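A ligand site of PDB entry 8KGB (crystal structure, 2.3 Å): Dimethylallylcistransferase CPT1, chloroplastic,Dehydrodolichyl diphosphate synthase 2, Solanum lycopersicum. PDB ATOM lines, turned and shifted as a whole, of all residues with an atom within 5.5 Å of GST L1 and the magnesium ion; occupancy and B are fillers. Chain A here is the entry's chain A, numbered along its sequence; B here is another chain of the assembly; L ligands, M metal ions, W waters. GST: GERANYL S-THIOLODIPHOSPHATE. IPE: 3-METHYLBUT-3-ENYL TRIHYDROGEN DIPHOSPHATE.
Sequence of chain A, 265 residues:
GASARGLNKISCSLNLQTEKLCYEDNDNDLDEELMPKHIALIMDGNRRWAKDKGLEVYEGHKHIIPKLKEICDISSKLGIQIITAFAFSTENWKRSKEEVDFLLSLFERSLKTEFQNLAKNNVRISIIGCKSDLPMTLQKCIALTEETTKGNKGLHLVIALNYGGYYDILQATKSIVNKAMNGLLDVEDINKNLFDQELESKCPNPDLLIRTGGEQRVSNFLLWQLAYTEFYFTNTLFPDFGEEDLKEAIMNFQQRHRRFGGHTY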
ATOM      1  N   MET A  43       2.846  14.135  12.216  1.00  0.00           N
ATOM      2  CA  MET A  43       1.637  14.875  11.743  1.00  0.00           C
ATOM      3  C   MET A  43       1.723  16.321  12.234  1.00  0.00           C
ATOM      4  O   MET A  43       1.018  16.692  13.199  1.00  0.00           O
ATOM      5  CB  MET A  43       0.361  14.174  12.211  1.00  0.00           C
ATOM      6  CG  MET A  43       0.310  12.714  11.720  1.00  0.00           C
ATOM      7  SD  MET A  43      -1.157  11.739  12.140  1.00  0.00           S
ATOM      8  CE  MET A  43      -1.111  11.800  13.942  1.00  0.00           C
ATOM      9  N   ASP A  44       2.593  17.101  11.584  1.00  0.00           N
ATOM     10  CA  ASP A  44       3.033  18.413  12.115  1.00  0.00           C
ATOM     11  C   ASP A  44       2.471  19.532  11.247  1.00  0.00           C
ATOM     12  O   ASP A  44       2.312  19.332  10.044  1.00  0.00           O
ATOM     13  CB  ASP A  44       4.561  18.495  12.185  1.00  0.00           C
ATOM     14  CG  ASP A  44       5.045  19.666  13.011  1.00  0.00           C
ATOM     15  OD1 ASP A  44       4.293  20.091  13.897  1.00  0.00           O
ATOM     16  OD2 ASP A  44       6.184  20.153  12.763  1.00  0.00           O
ATOM     17  N   GLY A  45       2.221  20.686  11.859  1.00  0.00           N
ATOM     18  CA  GLY A  45       1.850  21.926  11.155  1.00  0.00           C
ATOM     19  C   GLY A  45       0.375  22.272  11.260  1.00  0.00           C
ATOM     20  O   GLY A  45      -0.075  23.119  10.480  1.00  0.00           O
ATOM     21  N   ASN A  46      -0.357  21.674  12.200  1.00  0.00           N
ATOM     22  CA  ASN A  46      -1.840  21.838  12.252  1.00  0.00           C
ATOM     23  C   ASN A  46      -2.204  23.231  12.773  1.00  0.00           C
ATOM     24  O   ASN A  46      -3.263  23.755  12.386  1.00  0.00           O
ATOM     25  CB  ASN A  46      -2.487  20.768  13.099  1.00  0.00           C
ATOM     26  CG  ASN A  46      -2.168  19.391  12.570  1.00  0.00           C
ATOM     27  OD1 ASN A  46      -2.428  19.102  11.407  1.00  0.00           O
ATOM     28  ND2 ASN A  46      -1.575  18.552  13.400  1.00  0.00           N
ATOM     29  N   ARG A  47      -1.394  23.806  13.656  1.00  0.00           N
ATOM     30  CA  ARG A  47      -1.696  25.154  14.180  1.00  0.00           C
ATOM     31  C   ARG A  47      -1.509  26.179  13.055  1.00  0.00           C
ATOM     32  O   ARG A  47      -2.412  27.005  12.846  1.00  0.00           O
ATOM     33  CB  ARG A  47      -0.839  25.455  15.394  1.00  0.00           C
ATOM     34  CG  ARG A  47      -1.263  26.736  16.083  1.00  0.00           C
ATOM     35  CD  ARG A  47      -0.776  26.842  17.505  1.00  0.00           C
ATOM     36  NE  ARG A  47       0.481  27.557  17.561  1.00  0.00           N
ATOM     37  CZ  ARG A  47       0.970  28.158  18.650  1.00  0.00           C
ATOM     38  NH1 ARG A  47       0.293  28.149  19.786  1.00  0.00           N
ATOM     39  NH2 ARG A  47       2.150  28.752  18.592  1.00  0.00           N
ATOM     40  N   ARG A  48      -0.399  26.111  12.332  1.00  0.00           N
ATOM     41  CA  ARG A  48      -0.058  27.110  11.306  1.00  0.00           C
ATOM     42  C   ARG A  48      -1.038  26.977  10.134  1.00  0.00           C
ATOM     43  O   ARG A  48      -1.268  27.985   9.432  1.00  0.00           O
ATOM     44  CB  ARG A  48       1.384  26.936  10.808  1.00  0.00           C
ATOM     45  CG  ARG A  48       2.447  27.334  11.815  1.00  0.00           C
ATOM     46  CD  ARG A  48       3.802  26.773  11.379  1.00  0.00           C
ATOM     47  NE  ARG A  48       3.986  25.376  11.767  1.00  0.00           N
ATOM     48  CZ  ARG A  48       4.865  24.522  11.239  1.00  0.00           C
ATOM     49  NH1 ARG A  48       5.659  24.906  10.253  1.00  0.00           N
ATOM     50  NH2 ARG A  48       4.941  23.278  11.682  1.00  0.00           N
ATOM     51  N   TRP A  49      -1.585  25.799   9.918  1.00  0.00           N
ATOM     52  CA  TRP A  49      -2.598  25.607   8.846  1.00  0.00           C
ATOM     53  C   TRP A  49      -3.837  26.436   9.170  1.00  0.00           C
ATOM     54  O   TRP A  49      -4.425  26.990   8.225  1.00  0.00           O
ATOM     55  CB  TRP A  49      -2.948  24.141   8.698  1.00  0.00           C
ATOM     56  CG  TRP A  49      -3.951  23.864   7.617  1.00  0.00           C
ATOM     57  CD1 TRP A  49      -3.691  23.548   6.319  1.00  0.00           C
ATOM     58  CD2 TRP A  49      -5.371  23.832   7.767  1.00  0.00           C
ATOM     59  NE1 TRP A  49      -4.864  23.334   5.640  1.00  0.00           N
ATOM     60  CE2 TRP A  49      -5.911  23.496   6.500  1.00  0.00           C
ATOM     61  CE3 TRP A  49      -6.255  24.062   8.836  1.00  0.00           C
ATOM     62  CZ2 TRP A  49      -7.279  23.376   6.286  1.00  0.00           C
ATOM     63  CZ3 TRP A  49      -7.601  23.939   8.618  1.00  0.00           C
ATOM     64  CH2 TRP A  49      -8.110  23.605   7.359  1.00  0.00           C
ATOM     65  N   HIS A  61      -6.273  20.799  14.032  1.00  0.00           N
ATOM     66  CA  HIS A  61      -6.147  19.512  14.761  1.00  0.00           C
ATOM     67  C   HIS A  61      -7.409  18.671  14.522  1.00  0.00           C
ATOM     68  O   HIS A  61      -7.322  17.430  14.630  1.00  0.00           O
ATOM     69  CB  HIS A  61      -5.913  19.730  16.252  1.00  0.00           C
ATOM     70  CG  HIS A  61      -4.617  20.399  16.549  1.00  0.00           C
ATOM     71  ND1 HIS A  61      -4.466  21.769  16.501  1.00  0.00           N
ATOM     72  CD2 HIS A  61      -3.419  19.896  16.914  1.00  0.00           C
ATOM     73  CE1 HIS A  61      -3.225  22.079  16.824  1.00  0.00           C
ATOM     74  NE2 HIS A  61      -2.562  20.939  17.064  1.00  0.00           N
ATOM     75  N   ILE A  64      -6.949  15.921  11.971  1.00  0.00           N
ATOM     76  CA  ILE A  64      -5.851  14.928  12.127  1.00  0.00           C
ATOM     77  C   ILE A  64      -6.397  13.529  11.805  1.00  0.00           C
ATOM     78  O   ILE A  64      -5.909  12.909  10.820  1.00  0.00           O
ATOM     79  CB  ILE A  64      -5.205  15.019  13.518  1.00  0.00           C
ATOM     80  CG1 ILE A  64      -4.364  16.289  13.622  1.00  0.00           C
ATOM     81  CG2 ILE A  64      -4.380  13.768  13.803  1.00  0.00           C
ATOM     82  CD1 ILE A  64      -3.931  16.649  15.018  1.00  0.00           C
ATOM     83  N   PHE A  86       2.598   9.913  14.659  1.00  0.00           N
ATOM     84  CA  PHE A  86       2.993  10.656  15.874  1.00  0.00           C
ATOM     85  C   PHE A  86       1.846  11.609  16.199  1.00  0.00           C
ATOM     86  O   PHE A  86       1.664  12.583  15.451  1.00  0.00           O
ATOM     87  CB  PHE A  86       4.324  11.371  15.673  1.00  0.00           C
ATOM     88  CG  PHE A  86       5.154  11.614  16.920  1.00  0.00           C
ATOM     89  CD1 PHE A  86       4.794  11.090  18.154  1.00  0.00           C
ATOM     90  CD2 PHE A  86       6.315  12.370  16.854  1.00  0.00           C
ATOM     91  CE1 PHE A  86       5.556  11.307  19.287  1.00  0.00           C
ATOM     92  CE2 PHE A  86       7.098  12.582  17.981  1.00  0.00           C
ATOM     93  CZ  PHE A  86       6.717  12.058  19.207  1.00  0.00           C
ATOM     94  N   ALA A  87       1.090  11.332  17.263  1.00  0.00           N
ATOM     95  CA  ALA A  87      -0.097  12.119  17.626  1.00  0.00           C
ATOM     96  C   ALA A  87       0.155  13.024  18.840  1.00  0.00           C
ATOM     97  O   ALA A  87      -0.452  14.099  18.886  1.00  0.00           O
ATOM     98  CB  ALA A  87      -1.267  11.218  17.882  1.00  0.00           C
ATOM     99  N   PHE A  88       0.981  12.589  19.796  1.00  0.00           N
ATOM    100  CA  PHE A  88       1.252  13.379  21.019  1.00  0.00           C
ATOM    101  C   PHE A  88       2.571  12.910  21.617  1.00  0.00           C
ATOM    102  O   PHE A  88       2.659  11.734  22.002  1.00  0.00           O
ATOM    103  CB  PHE A  88       0.088  13.235  21.994  1.00  0.00           C
ATOM    104  CG  PHE A  88       0.237  13.944  23.320  1.00  0.00           C
ATOM    105  CD1 PHE A  88       0.444  15.309  23.373  1.00  0.00           C
ATOM    106  CD2 PHE A  88       0.135  13.249  24.512  1.00  0.00           C
ATOM    107  CE1 PHE A  88       0.575  15.954  24.592  1.00  0.00           C
ATOM    108  CE2 PHE A  88       0.254  13.900  25.735  1.00  0.00           C
ATOM    109  CZ  PHE A  88       0.495  15.251  25.766  1.00  0.00           C
ATOM    110  N   ASN A  92       5.238  17.505  24.512  1.00  0.00           N
ATOM    111  CA  ASN A  92       4.048  18.365  24.284  1.00  0.00           C
ATOM    112  C   ASN A  92       3.387  18.725  25.628  1.00  0.00           C
ATOM    113  O   ASN A  92       2.666  19.720  25.686  1.00  0.00           O
ATOM    114  CB  ASN A  92       3.066  17.725  23.294  1.00  0.00           C
ATOM    115  CG  ASN A  92       3.535  17.668  21.854  1.00  0.00           C
ATOM    116  OD1 ASN A  92       3.222  16.733  21.139  1.00  0.00           O
ATOM    117  ND2 ASN A  92       4.259  18.679  21.382  1.00  0.00           N
ATOM    118  N   ARG A  95       3.299  22.468  26.732  1.00  0.00           N
ATOM    119  CA  ARG A  95       2.301  23.436  26.247  1.00  0.00           C
ATOM    120  C   ARG A  95       1.331  23.774  27.381  1.00  0.00           C
ATOM    121  O   ARG A  95       1.440  23.173  28.486  1.00  0.00           O
ATOM    122  CB  ARG A  95       1.598  22.888  25.003  1.00  0.00           C
ATOM    123  CG  ARG A  95       2.549  22.624  23.852  1.00  0.00           C
ATOM    124  CD  ARG A  95       1.908  21.963  22.656  1.00  0.00           C
ATOM    125  NE  ARG A  95       2.874  21.730  21.584  1.00  0.00           N
ATOM    126  CZ  ARG A  95       2.577  21.454  20.310  1.00  0.00           C
ATOM    127  NH1 ARG A  95       1.322  21.358  19.924  1.00  0.00           N
ATOM    128  NH2 ARG A  95       3.549  21.260  19.435  1.00  0.00           N
ATOM    129  N   GLU A  99      -4.365  23.975  26.082  1.00  0.00           N
ATOM    130  CA  GLU A  99      -4.105  23.285  24.795  1.00  0.00           C
ATOM    131  C   GLU A  99      -4.113  21.771  25.032  1.00  0.00           C
ATOM    132  O   GLU A  99      -4.793  21.030  24.308  1.00  0.00           O
ATOM    133  CB  GLU A  99      -2.802  23.731  24.145  1.00  0.00           C
ATOM    134  CG  GLU A  99      -2.526  22.976  22.858  1.00  0.00           C
ATOM    135  CD  GLU A  99      -1.427  23.555  21.966  1.00  0.00           C
ATOM    136  OE1 GLU A  99      -0.864  24.604  22.352  1.00  0.00           O
ATOM    137  OE2 GLU A  99      -1.180  22.977  20.880  1.00  0.00           O
ATOM    138  N   VAL A 100      -3.402  21.312  26.049  1.00  0.00           N
ATOM    139  CA  VAL A 100      -3.287  19.847  26.292  1.00  0.00           C
ATOM    140  C   VAL A 100      -4.694  19.274  26.561  1.00  0.00           C
ATOM    141  O   VAL A 100      -5.037  18.267  25.927  1.00  0.00           O
ATOM    142  CB  VAL A 100      -2.313  19.545  27.435  1.00  0.00           C
ATOM    143  CG1 VAL A 100      -2.347  18.066  27.794  1.00  0.00           C
ATOM    144  CG2 VAL A 100      -0.916  19.973  27.042  1.00  0.00           C
ATOM    145  N   LEU A 103      -6.861  19.326  23.281  1.00  0.00           N
ATOM    146  CA  LEU A 103      -6.446  18.370  22.224  1.00  0.00           C
ATOM    147  C   LEU A 103      -6.564  16.916  22.719  1.00  0.00           C
ATOM    148  O   LEU A 103      -6.888  16.057  21.896  1.00  0.00           O
ATOM    149  CB  LEU A 103      -5.020  18.717  21.755  1.00  0.00           C
ATOM    150  CG  LEU A 103      -4.888  19.530  20.458  1.00  0.00           C
ATOM    151  CD1 LEU A 103      -6.192  20.155  19.966  1.00  0.00           C
ATOM    152  CD2 LEU A 103      -3.822  20.603  20.602  1.00  0.00           C
ATOM    153  N   LEU A 104      -6.349  16.614  24.008  1.00  0.00           N
ATOM    154  CA  LEU A 104      -6.610  15.235  24.493  1.00  0.00           C
ATOM    155  C   LEU A 104      -8.110  14.920  24.441  1.00  0.00           C
ATOM    156  O   LEU A 104      -8.458  13.792  24.063  1.00  0.00           O
ATOM    157  CB  LEU A 104      -6.039  15.049  25.897  1.00  0.00           C
ATOM    158  CG  LEU A 104      -4.522  14.929  25.973  1.00  0.00           C
ATOM    159  CD1 LEU A 104      -4.059  14.597  27.390  1.00  0.00           C
ATOM    160  CD2 LEU A 104      -3.992  13.892  24.994  1.00  0.00           C
ATOM    161  N   LEU A 161       1.099   8.031  21.273  1.00  0.00           N
ATOM    162  CA  LEU A 161       0.292   8.962  22.108  1.00  0.00           C
ATOM    163  C   LEU A 161       0.904   9.022  23.500  1.00  0.00           C
ATOM    164  O   LEU A 161       0.957   7.974  24.154  1.00  0.00           O
ATOM    165  CB  LEU A 161      -1.139   8.458  22.122  1.00  0.00           C
ATOM    166  CG  LEU A 161      -2.202   9.427  22.610  1.00  0.00           C
ATOM    167  CD1 LEU A 161      -2.333  10.635  21.699  1.00  0.00           C
ATOM    168  CD2 LEU A 161      -3.518   8.679  22.703  1.00  0.00           C
ATOM    169  N   ARG A 211       7.526  13.538   7.254  1.00  0.00           N
ATOM    170  CA  ARG A 211       7.210  14.620   8.200  1.00  0.00           C
ATOM    171  C   ARG A 211       6.649  15.785   7.399  1.00  0.00           C
ATOM    172  O   ARG A 211       7.377  16.327   6.544  1.00  0.00           O
ATOM    173  CB  ARG A 211       8.432  15.062   9.015  1.00  0.00           C
ATOM    174  CG  ARG A 211       8.112  16.240   9.929  1.00  0.00           C
ATOM    175  CD  ARG A 211       9.180  16.501  10.960  1.00  0.00           C
ATOM    176  NE  ARG A 211       8.773  17.569  11.868  1.00  0.00           N
ATOM    177  CZ  ARG A 211       9.019  17.602  13.167  1.00  0.00           C
ATOM    178  NH1 ARG A 211       9.737  16.647  13.744  1.00  0.00           N
ATOM    179  NH2 ARG A 211       8.582  18.608  13.894  1.00  0.00           N
ATOM    180  N   ARG B 259      11.502  24.509  18.676  1.00  0.00           N
ATOM    181  CA  ARG B 259      10.413  24.646  19.675  1.00  0.00           C
ATOM    182  C   ARG B 259      10.524  23.581  20.770  1.00  0.00           C
ATOM    183  O   ARG B 259      10.004  23.846  21.869  1.00  0.00           O
ATOM    184  CB  ARG B 259       9.058  24.585  18.973  1.00  0.00           C
ATOM    185  CG  ARG B 259       8.776  25.728  18.008  1.00  0.00           C
ATOM    186  CD  ARG B 259       7.514  25.487  17.184  1.00  0.00           C
ATOM    187  NE  ARG B 259       7.761  25.956  15.828  1.00  0.00           N
ATOM    188  CZ  ARG B 259       7.602  25.226  14.718  1.00  0.00           C
ATOM    189  NH1 ARG B 259       7.091  24.015  14.761  1.00  0.00           N
ATOM    190  NH2 ARG B 259       7.922  25.754  13.548  1.00  0.00           N
ATOM    191  N   HIS B 263       5.180  25.669  22.685  1.00  0.00           N
ATOM    192  CA  HIS B 263       4.415  26.659  21.886  1.00  0.00           C
ATOM    193  C   HIS B 263       4.574  28.068  22.460  1.00  0.00           C
ATOM    194  O   HIS B 263       4.759  28.210  23.697  1.00  0.00           O
ATOM    195  CB  HIS B 263       2.924  26.306  21.825  1.00  0.00           C
ATOM    196  CG  HIS B 263       2.513  25.660  20.547  1.00  0.00           C
ATOM    197  ND1 HIS B 263       1.319  24.980  20.431  1.00  0.00           N
ATOM    198  CD2 HIS B 263       3.115  25.590  19.328  1.00  0.00           C
ATOM    199  CE1 HIS B 263       1.193  24.516  19.197  1.00  0.00           C
ATOM    200  NE2 HIS B 263       2.282  24.867  18.500  1.00  0.00           N
HETATM  201  PA  GST L   1       2.460  23.624  14.520  1.00  0.00           P
HETATM  202  O1A GST L   1       1.843  24.305  13.316  1.00  0.00           O
HETATM  203  O2A GST L   1       3.648  22.787  14.167  1.00  0.00           O
HETATM  204  O3A GST L   1       2.711  24.525  15.698  1.00  0.00           O
HETATM  205  O1B GST L   1       1.320  22.583  14.973  1.00  0.00           O
HETATM  206  PB  GST L   1       1.381  21.473  16.110  1.00  0.00           P
HETATM  207  O2B GST L   1       2.795  21.318  16.610  1.00  0.00           O
HETATM  208  O3B GST L   1       0.378  21.770  17.173  1.00  0.00           O
HETATM  209  S1  GST L   1       0.843  19.823  14.961  1.00  0.00           S
HETATM  210  C1  GST L   1       1.933  18.550  15.655  1.00  0.00           C
HETATM  211  C2  GST L   1       1.645  18.297  17.087  1.00  0.00           C
HETATM  212  C3  GST L   1       0.585  17.636  17.531  1.00  0.00           C
HETATM  213  C10 GST L   1      -0.472  17.060  16.628  1.00  0.00           C
HETATM  214  C4  GST L   1       0.352  17.415  18.993  1.00  0.00           C
HETATM  215  C5  GST L   1      -1.038  17.828  19.430  1.00  0.00           C
HETATM  216  C6  GST L   1      -1.146  18.054  20.908  1.00  0.00           C
HETATM  217  C7  GST L   1      -1.845  17.362  21.799  1.00  0.00           C
HETATM  218  C9  GST L   1      -1.960  17.779  23.235  1.00  0.00           C
HETATM  219  C8  GST L   1      -2.580  16.096  21.445  1.00  0.00           C
HETATM  220  C1  IPE L   2       5.259  17.108  16.228  1.00  0.00           C
HETATM  221  O1  IPE L   2       6.437  17.826  16.465  1.00  0.00           O
HETATM  222  C2  IPE L   2       4.996  16.179  17.354  1.00  0.00           C
HETATM  223  C3  IPE L   2       3.759  15.400  17.030  1.00  0.00           C
HETATM  224  C4  IPE L   2       3.308  15.330  15.776  1.00  0.00           C
HETATM  225  C5  IPE L   2       3.039  14.777  18.180  1.00  0.00           C
HETATM  226  PA  IPE L   2       6.400  19.111  17.412  1.00  0.00           P
HETATM  227  O1A IPE L   2       6.160  18.746  18.838  1.00  0.00           O
HETATM  228  O2A IPE L   2       5.618  20.188  16.746  1.00  0.00           O
HETATM  229  O3A IPE L   2       7.974  19.361  17.288  1.00  0.00           O
HETATM  230  PB  IPE L   2       8.981  20.580  17.366  1.00  0.00           P
HETATM  231  O1B IPE L   2       8.632  21.384  16.135  1.00  0.00           O
HETATM  232  O2B IPE L   2      10.352  19.959  17.324  1.00  0.00           O
HETATM  233  O3B IPE L   2       8.692  21.267  18.689  1.00  0.00           O
HETATM  234 MG    MG M   1       4.512  21.453  15.435  1.00  0.00          MG
HETATM  235  O   HOH W   1       2.482  27.782  15.560  1.00  0.00           O
HETATM  236  O   HOH W   2       6.589  21.802  14.658  1.00  0.00           O
HETATM  237  O   HOH W   3       5.075  23.067  16.776  1.00  0.00           O
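O1A of GST L1 sits at hydrogen-bond distance from N of Arg 48.
O1A of GST L1 is in salt-bridge range of NE of Arg 48 (2.9 Å).
A ring nitrogen (NE2) of His 263 of chain B sits at hydrogen-bond distance from an oxygen (O3A) of GST L1, at 2.9 Å.
The guanidinium group (NH1) of Arg 95 lies within salt-bridge range of an oxygen (O3B) of GST L1, at 2.9 Å.
A ring nitrogen (NE2) of His 61 sits at hydrogen-bond distance from an oxygen (O3B) of GST L1 (3.1 Å).
An oxygen (O1B) of GST L1 lies within hydrogen-bond range of the backbone NH of Asn 46 (3.4 Å).
The side-chain amide nitrogen of Asn 46 lies close to a sulfur (S1) of GST L1, at 3.1 Å.
S1 of GST L1 sits close to N of Gly 45 (3.5 Å).
An oxygen (O1B) of GST L1 is in hydrogen-bond range of the backbone NH (N) of Arg 47 (3.3 Å).
The guanidinium group (NH1) of Arg 259 of chain B lies close to an oxygen (O2A) of GST L1 (3.7 Å).
The guanidinium group (NH2) of Arg 95 is in salt-bridge range of an oxygen (O1A) of IPE L2.
ND2 of Asn 92 lies within hydrogen-bond range of O1A of IPE L2 (3.2 Å).
The guanidinium group (NH1) of Arg 259 of chain B is in salt-bridge range of an oxygen (O1B) of IPE L2, 3.3 Å away.
O1B of IPE L2 is in salt-bridge range of NH2 of Arg 211.
The side-chain carboxylate of Asp 44 lies within salt-bridge range of the guanidinium group of Arg 48 (3.5 Å).
The side-chain carboxylate (OD2) of Asp 44 is in salt-bridge range of the guanidinium group (NH2) of Arg 211 (3.1 Å).
A ring nitrogen (NE2) of His 263 of chain B lies within hydrogen-bond range of the guanidinium group of Arg 47, 3.4 Å away.
A ring nitrogen (ND1) of His 263 of chain B lies within hydrogen-bond range of the side-chain carboxylate (OE1) of Glu 99 (2.9 Å).
The guanidinium group (NH2) of Arg 95 sits close to the side-chain amide nitrogen (ND2) of Asn 92 (3.3 Å).
The guanidinium group (NH1) of Arg 95 lies within salt-bridge range of the side-chain carboxylate (OE2) of Glu 99 (3.1 Å).
ND2 of Asn 46 is in hydrogen-bond range of O of Met 43 (3.2 Å).
O of Met 43 lies close to S1 of GST L1 (3.6 Å).
Merely in contact with GST L1: Phe 88 (3.4 Å), Ala 87 (3.4 Å), Leu 103 (3.5 Å), Asn 92 (3.6 Å), Ile 64 (3.8 Å) and Val 100 (3.9 Å).
Hydrophobic or aromatic side chains that line GST L1: His 61, Ile 64, Phe 88, Leu 103 and His 263 of chain B.
Of the 22 residues printed, 16 come within 4 Å of GST L1.
Residues that only touch the magnesium ion: Arg 259 of chain B.
The magnesium ion is bound by an oxygen (O2A) of GST L1 (2.0 Å), the side-chain carboxylate of Asp 44 (2.1 Å), an oxygen (O2B) of GST L1 (2.1 Å), an oxygen (O2A) of IPE L2 (2.1 Å), water W3 (2.2 Å) and water W2 (2.2 Å).
The magnesium ion has six donor atoms within binding distance.
Water W3 bridges an oxygen (O3A) of GST L1 and the guanidinium group (NH1) of Arg 259 of chain B.
Water W2 lies within hydrogen-bond range of OD2 of Asp 44 (2.5 Å) and O1B of IPE L2 (2.6 Å).
Water W1 lies within hydrogen-bond range of the guanidinium group (NE) of Arg 47 (2.8 Å) and an oxygen (O3A) of GST L1 (3.3 Å).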
